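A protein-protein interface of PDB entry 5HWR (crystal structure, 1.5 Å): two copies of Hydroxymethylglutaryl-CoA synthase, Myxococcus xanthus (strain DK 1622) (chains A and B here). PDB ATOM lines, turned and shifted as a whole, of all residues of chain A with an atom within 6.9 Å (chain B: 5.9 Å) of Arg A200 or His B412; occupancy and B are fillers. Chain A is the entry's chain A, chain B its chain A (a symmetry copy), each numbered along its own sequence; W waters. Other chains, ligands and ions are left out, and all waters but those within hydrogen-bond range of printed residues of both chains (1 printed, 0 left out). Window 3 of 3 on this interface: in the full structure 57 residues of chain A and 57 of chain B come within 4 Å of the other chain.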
ATOM      1  N   TYR A 192     -22.890  36.429  35.044  1.00  0.00           N
ATOM      2  CA  TYR A 192     -23.212  35.035  34.788  1.00  0.00           C
ATOM      3  C   TYR A 192     -23.150  34.215  36.067  1.00  0.00           C
ATOM      4  O   TYR A 192     -22.308  33.330  36.212  1.00  0.00           O
ATOM      5  CB  TYR A 192     -22.268  34.485  33.718  1.00  0.00           C
ATOM      6  CG  TYR A 192     -22.784  34.578  32.289  1.00  0.00           C
ATOM      7  CD1 TYR A 192     -23.975  33.984  31.935  1.00  0.00           C
ATOM      8  CD2 TYR A 192     -22.045  35.180  31.283  1.00  0.00           C
ATOM      9  CE1 TYR A 192     -24.435  33.994  30.611  1.00  0.00           C
ATOM     10  CE2 TYR A 192     -22.501  35.205  29.959  1.00  0.00           C
ATOM     11  CZ  TYR A 192     -23.685  34.603  29.637  1.00  0.00           C
ATOM     12  OH  TYR A 192     -24.147  34.571  28.349  1.00  0.00           O
ATOM     13  N   TRP A 195     -27.781  30.907  34.847  1.00  0.00           N
ATOM     14  CA  TRP A 195     -28.463  31.146  33.585  1.00  0.00           C
ATOM     15  C   TRP A 195     -28.921  29.799  33.048  1.00  0.00           C
ATOM     16  O   TRP A 195     -28.540  28.744  33.561  1.00  0.00           O
ATOM     17  CB  TRP A 195     -27.572  31.919  32.604  1.00  0.00           C
ATOM     18  CG  TRP A 195     -26.372  31.231  32.022  1.00  0.00           C
ATOM     19  CD1 TRP A 195     -26.217  30.876  30.715  1.00  0.00           C
ATOM     20  CD2 TRP A 195     -25.126  30.900  32.674  1.00  0.00           C
ATOM     21  NE1 TRP A 195     -24.974  30.310  30.514  1.00  0.00           N
ATOM     22  CE2 TRP A 195     -24.285  30.320  31.694  1.00  0.00           C
ATOM     23  CE3 TRP A 195     -24.629  31.040  33.990  1.00  0.00           C
ATOM     24  CZ2 TRP A 195     -22.985  29.892  31.977  1.00  0.00           C
ATOM     25  CZ3 TRP A 195     -23.334  30.585  34.258  1.00  0.00           C
ATOM     26  CH2 TRP A 195     -22.545  30.013  33.254  1.00  0.00           C
ATOM     27  N   ARG A 196     -29.762  29.831  32.019  1.00  0.00           N
ATOM     28  CA  ARG A 196     -30.292  28.594  31.444  1.00  0.00           C
ATOM     29  C   ARG A 196     -30.533  28.805  29.950  1.00  0.00           C
ATOM     30  O   ARG A 196     -31.599  29.286  29.534  1.00  0.00           O
ATOM     31  CB  ARG A 196     -31.573  28.157  32.152  1.00  0.00           C
ATOM     32  CG  ARG A 196     -31.966  26.765  31.783  1.00  0.00           C
ATOM     33  CD  ARG A 196     -33.036  26.197  32.686  1.00  0.00           C
ATOM     34  NE  ARG A 196     -34.323  26.893  32.660  1.00  0.00           N
ATOM     35  CZ  ARG A 196     -35.339  26.560  31.881  1.00  0.00           C
ATOM     36  NH1 ARG A 196     -35.219  25.583  30.996  1.00  0.00           N
ATOM     37  NH2 ARG A 196     -36.486  27.214  32.001  1.00  0.00           N
ATOM     38  N   PRO A 197     -29.555  28.445  29.112  1.00  0.00           N
ATOM     39  CA  PRO A 197     -29.694  28.641  27.666  1.00  0.00           C
ATOM     40  C   PRO A 197     -30.939  27.972  27.103  1.00  0.00           C
ATOM     41  O   PRO A 197     -31.435  26.968  27.621  1.00  0.00           O
ATOM     42  CB  PRO A 197     -28.414  27.983  27.116  1.00  0.00           C
ATOM     43  CG  PRO A 197     -27.419  28.214  28.196  1.00  0.00           C
ATOM     44  CD  PRO A 197     -28.175  28.057  29.470  1.00  0.00           C
ATOM     45  N   VAL A 198     -31.427  28.550  26.018  1.00  0.00           N
ATOM     46  CA  VAL A 198     -32.644  28.061  25.381  1.00  0.00           C
ATOM     47  C   VAL A 198     -32.532  26.584  25.081  1.00  0.00           C
ATOM     48  O   VAL A 198     -31.570  26.129  24.455  1.00  0.00           O
ATOM     49  CB  VAL A 198     -32.925  28.846  24.097  1.00  0.00           C
ATOM     50  CG1 VAL A 198     -33.990  28.123  23.288  1.00  0.00           C
ATOM     51  CG2 VAL A 198     -33.335  30.232  24.465  1.00  0.00           C
ATOM     52  N   GLY A 199     -33.568  25.843  25.447  1.00  0.00           N
ATOM     53  CA  GLY A 199     -33.610  24.434  25.190  1.00  0.00           C
ATOM     54  C   GLY A 199     -32.926  23.575  26.228  1.00  0.00           C
ATOM     55  O   GLY A 199     -33.202  22.365  26.279  1.00  0.00           O
ATOM     56  N   ARG A 200     -32.078  24.162  27.082  1.00  0.00           N
ATOM     57  CA  ARG A 200     -31.472  23.422  28.176  1.00  0.00           C
ATOM     58  C   ARG A 200     -32.484  23.331  29.301  1.00  0.00           C
ATOM     59  O   ARG A 200     -32.915  24.362  29.814  1.00  0.00           O
ATOM     60  CB  ARG A 200     -30.206  24.118  28.656  1.00  0.00           C
ATOM     61  CG  ARG A 200     -29.326  23.190  29.399  1.00  0.00           C
ATOM     62  CD  ARG A 200     -28.189  23.928  30.090  1.00  0.00           C
ATOM     63  NE  ARG A 200     -27.383  23.017  30.895  1.00  0.00           N
ATOM     64  CZ  ARG A 200     -26.353  22.324  30.419  1.00  0.00           C
ATOM     65  NH1 ARG A 200     -25.657  21.544  31.238  1.00  0.00           N
ATOM     66  NH2 ARG A 200     -26.013  22.410  29.127  1.00  0.00           N
ATOM     67  N   ARG A 201     -32.835  22.119  29.718  1.00  0.00           N
ATOM     68  CA  ARG A 201     -33.853  21.975  30.749  1.00  0.00           C
ATOM     69  C   ARG A 201     -33.338  22.326  32.125  1.00  0.00           C
ATOM     70  O   ARG A 201     -34.125  22.721  32.989  1.00  0.00           O
ATOM     71  CB  ARG A 201     -34.394  20.551  30.767  1.00  0.00           C
ATOM     72  CG  ARG A 201     -35.716  20.454  30.125  1.00  0.00           C
ATOM     73  CD  ARG A 201     -36.254  19.068  30.274  1.00  0.00           C
ATOM     74  NE  ARG A 201     -37.536  19.033  30.960  1.00  0.00           N
ATOM     75  CZ  ARG A 201     -38.146  17.890  31.235  1.00  0.00           C
ATOM     76  NH1 ARG A 201     -37.531  16.762  30.908  1.00  0.00           N
ATOM     77  NH2 ARG A 201     -39.333  17.873  31.841  1.00  0.00           N
ATOM     78  N   GLU A 202     -32.039  22.163  32.357  1.00  0.00           N
ATOM     79  CA  GLU A 202     -31.446  22.362  33.669  1.00  0.00           C
ATOM     80  C   GLU A 202     -30.557  23.595  33.676  1.00  0.00           C
ATOM     81  O   GLU A 202     -29.881  23.894  32.692  1.00  0.00           O
ATOM     82  CB  GLU A 202     -30.650  21.129  34.071  1.00  0.00           C
ATOM     83  CG  GLU A 202     -31.600  20.011  34.422  1.00  0.00           C
ATOM     84  CD  GLU A 202     -31.005  18.628  34.405  1.00  0.00           C
ATOM     85  OE1 GLU A 202     -29.753  18.488  34.364  1.00  0.00           O
ATOM     86  OE2 GLU A 202     -31.837  17.689  34.448  1.00  0.00           O
ATOM     87  N   ALA A 203     -30.560  24.293  34.797  1.00  0.00           N
ATOM     88  CA  ALA A 203     -29.821  25.537  34.926  1.00  0.00           C
ATOM     89  C   ALA A 203     -28.320  25.295  35.032  1.00  0.00           C
ATOM     90  O   ALA A 203     -27.845  24.226  35.430  1.00  0.00           O
ATOM     91  CB  ALA A 203     -30.304  26.303  36.149  1.00  0.00           C
ATOM     92  N   LEU A 204     -27.586  26.324  34.662  1.00  0.00           N
ATOM     93  CA  LEU A 204     -26.154  26.448  34.911  1.00  0.00           C
ATOM     94  C   LEU A 204     -25.965  27.456  36.035  1.00  0.00           C
ATOM     95  O   LEU A 204     -26.615  28.510  36.040  1.00  0.00           O
ATOM     96  CB  LEU A 204     -25.440  26.918  33.645  1.00  0.00           C
ATOM     97  CG  LEU A 204     -25.575  25.971  32.460  1.00  0.00           C
ATOM     98  CD1 LEU A 204     -25.177  26.666  31.163  1.00  0.00           C
ATOM     99  CD2 LEU A 204     -24.706  24.764  32.698  1.00  0.00           C
ATOM    100  N   HIS B  90     -33.529  31.327  29.046  1.00  0.00           N
ATOM    101  CA  HIS B  90     -34.777  31.234  29.792  1.00  0.00           C
ATOM    102  C   HIS B  90     -34.792  32.155  30.999  1.00  0.00           C
ATOM    103  O   HIS B  90     -35.864  32.492  31.500  1.00  0.00           O
ATOM    104  CB  HIS B  90     -35.013  29.810  30.261  1.00  0.00           C
ATOM    105  CG  HIS B  90     -35.368  28.859  29.177  1.00  0.00           C
ATOM    106  ND1 HIS B  90     -36.610  28.865  28.595  1.00  0.00           N
ATOM    107  CD2 HIS B  90     -34.673  27.861  28.579  1.00  0.00           C
ATOM    108  CE1 HIS B  90     -36.664  27.909  27.683  1.00  0.00           C
ATOM    109  NE2 HIS B  90     -35.509  27.277  27.662  1.00  0.00           N
ATOM    110  N   ILE B 409     -19.869  31.401  21.612  1.00  0.00           N
ATOM    111  CA  ILE B 409     -20.368  30.926  22.885  1.00  0.00           C
ATOM    112  C   ILE B 409     -19.297  29.994  23.432  1.00  0.00           C
ATOM    113  O   ILE B 409     -18.865  29.061  22.745  1.00  0.00           O
ATOM    114  CB  ILE B 409     -21.731  30.234  22.749  1.00  0.00           C
ATOM    115  CG1 ILE B 409     -22.746  31.210  22.143  1.00  0.00           C
ATOM    116  CG2 ILE B 409     -22.198  29.759  24.119  1.00  0.00           C
ATOM    117  CD1 ILE B 409     -24.134  30.658  21.925  1.00  0.00           C
ATOM    118  N   ARG B 410     -18.813  30.294  24.633  1.00  0.00           N
ATOM    119  CA  ARG B 410     -17.701  29.564  25.220  1.00  0.00           C
ATOM    120  C   ARG B 410     -18.141  29.154  26.610  1.00  0.00           C
ATOM    121  O   ARG B 410     -18.510  30.013  27.418  1.00  0.00           O
ATOM    122  CB  ARG B 410     -16.429  30.422  25.256  1.00  0.00           C
ATOM    123  N   ASP B 411     -18.136  27.846  26.877  1.00  0.00           N
ATOM    124  CA  ASP B 411     -18.560  27.349  28.180  1.00  0.00           C
ATOM    125  C   ASP B 411     -19.963  27.863  28.500  1.00  0.00           C
ATOM    126  O   ASP B 411     -20.263  28.268  29.626  1.00  0.00           O
ATOM    127  CB  ASP B 411     -17.549  27.757  29.264  1.00  0.00           C
ATOM    128  N   HIS B 412     -20.825  27.870  27.481  1.00  0.00           N
ATOM    129  CA  HIS B 412     -22.218  28.321  27.546  1.00  0.00           C
ATOM    130  C   HIS B 412     -22.383  29.809  27.818  1.00  0.00           C
ATOM    131  O   HIS B 412     -23.525  30.271  28.023  1.00  0.00           O
ATOM    132  CB  HIS B 412     -23.006  27.537  28.601  1.00  0.00           C
ATOM    133  CG  HIS B 412     -22.935  26.061  28.407  1.00  0.00           C
ATOM    134  ND1 HIS B 412     -22.075  25.261  29.123  1.00  0.00           N
ATOM    135  CD2 HIS B 412     -23.599  25.243  27.559  1.00  0.00           C
ATOM    136  CE1 HIS B 412     -22.226  24.005  28.737  1.00  0.00           C
ATOM    137  NE2 HIS B 412     -23.148  23.968  27.790  1.00  0.00           N
ATOM    138  N   ARG B 413     -21.303  30.589  27.793  1.00  0.00           N
ATOM    139  CA  ARG B 413     -21.361  32.028  28.006  1.00  0.00           C
ATOM    140  C   ARG B 413     -21.232  32.737  26.664  1.00  0.00           C
ATOM    141  O   ARG B 413     -20.292  32.483  25.896  1.00  0.00           O
ATOM    142  CB  ARG B 413     -20.262  32.497  28.971  1.00  0.00           C
ATOM    143  CG  ARG B 413     -20.383  31.977  30.410  1.00  0.00           C
ATOM    144  CD  ARG B 413     -19.126  32.428  31.209  1.00  0.00           C
ATOM    145  NE  ARG B 413     -19.128  31.995  32.601  1.00  0.00           N
ATOM    146  CZ  ARG B 413     -18.828  30.764  32.992  1.00  0.00           C
ATOM    147  NH1 ARG B 413     -18.533  29.842  32.077  1.00  0.00           N
ATOM    148  NH2 ARG B 413     -18.870  30.445  34.285  1.00  0.00           N
ATOM    149  N   ARG B 414     -22.167  33.620  26.387  1.00  0.00           N
ATOM    150  CA  ARG B 414     -22.168  34.368  25.141  1.00  0.00           C
ATOM    151  C   ARG B 414     -21.153  35.491  25.217  1.00  0.00           C
ATOM    152  O   ARG B 414     -21.107  36.239  26.206  1.00  0.00           O
ATOM    153  CB  ARG B 414     -23.558  34.941  24.875  1.00  0.00           C
ATOM    154  CG  ARG B 414     -24.626  33.860  24.860  1.00  0.00           C
ATOM    155  CD  ARG B 414     -26.024  34.411  24.774  1.00  0.00           C
ATOM    156  NE  ARG B 414     -26.380  34.819  23.433  1.00  0.00           N
ATOM    157  CZ  ARG B 414     -26.876  34.006  22.499  1.00  0.00           C
ATOM    158  NH1 ARG B 414     -27.074  32.707  22.750  1.00  0.00           N
ATOM    159  NH2 ARG B 414     -27.190  34.502  21.314  1.00  0.00           N
HETATM  160  O   HOH W   1     -19.767  32.485  35.696  1.00  0.00           O
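Of the printed residues of chain B, Trp A195 touches Asp B411, His B412 and Arg B413.
Of the printed residues of chain B, Pro A197 touches His B90.
Printed residues of chain B within 4 Å of Gly A199: His B90.
Of chain B, only His B412 comes within 4 Å of Arg A200.
The nearest residue of chain B that does not touch Arg A200 is His B90 (4.1 Å).
The nearest residue of chain A that does not touch His B412 is Tyr A192 (4.4 Å).
No position is printed for both chains.
Of the 11 pairs that touch across the chains among the printed residues, none has its exchanged pair printed and touching as well.
Water W1 lies within hydrogen-bond range of the guanidinium group of Arg B413 (2.6 Å) and the backbone carbonyl oxygen of Tyr A192 (2.7 Å).
Tyr A192 touches Arg B413.
Trp A195 touches Asp B411 (CZ2 to O, 3.9 Å).
Arg B413 touches Trp A195.
Pro A197 touches His B90.
NE2 of His B90 touches CA of Val A198, 3.7 Å away.
Arg A200 touches His B412 (NH2 to NE2, 3.5 Å).
CD1 of Leu A204 touches CB of His B412 (3.5 Å).
Of the 11 printed residues of chain A, 8 touch a printed residue of chain B.
Hydrophobic or aromatic side chains of chain A that line the printed part of chain B: Tyr A192, Trp A195 and Leu A204.
Hydrophobic or aromatic side chains of chain B that line the printed part of chain A: His B90 and His B412.
The guanidinium group of Arg A200 sits close to the backbone carbonyl oxygen of Glu A202.
The backbone carbonyl oxygen (O) of Asp B411 is in hydrogen-bond range of the guanidinium group (NH1) of Arg B413 (3.4 Å).
The guanidinium group (NH1) of Arg A196 lies within hydrogen-bond range of the backbone carbonyl oxygen (O) of Arg A200.
The backbone NH (N) of Leu A204 is in hydrogen-bond range of the backbone carbonyl oxygen (O) of Trp A195.
A ring nitrogen (NE2) of His B90 is in hydrogen-bond range of the backbone NH of Gly A199 (3.3 Å).
The backbone NH (N) of His B90 sits at hydrogen-bond distance from the backbone carbonyl oxygen (O) of Arg A196 (2.9 Å).
The backbone carbonyl oxygen (O) of His B412 lies within hydrogen-bond range of the indole nitrogen (NE1) of Trp A195, 2.9 Å away.
OH of Tyr A192 is in hydrogen-bond range of N of Arg B414.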
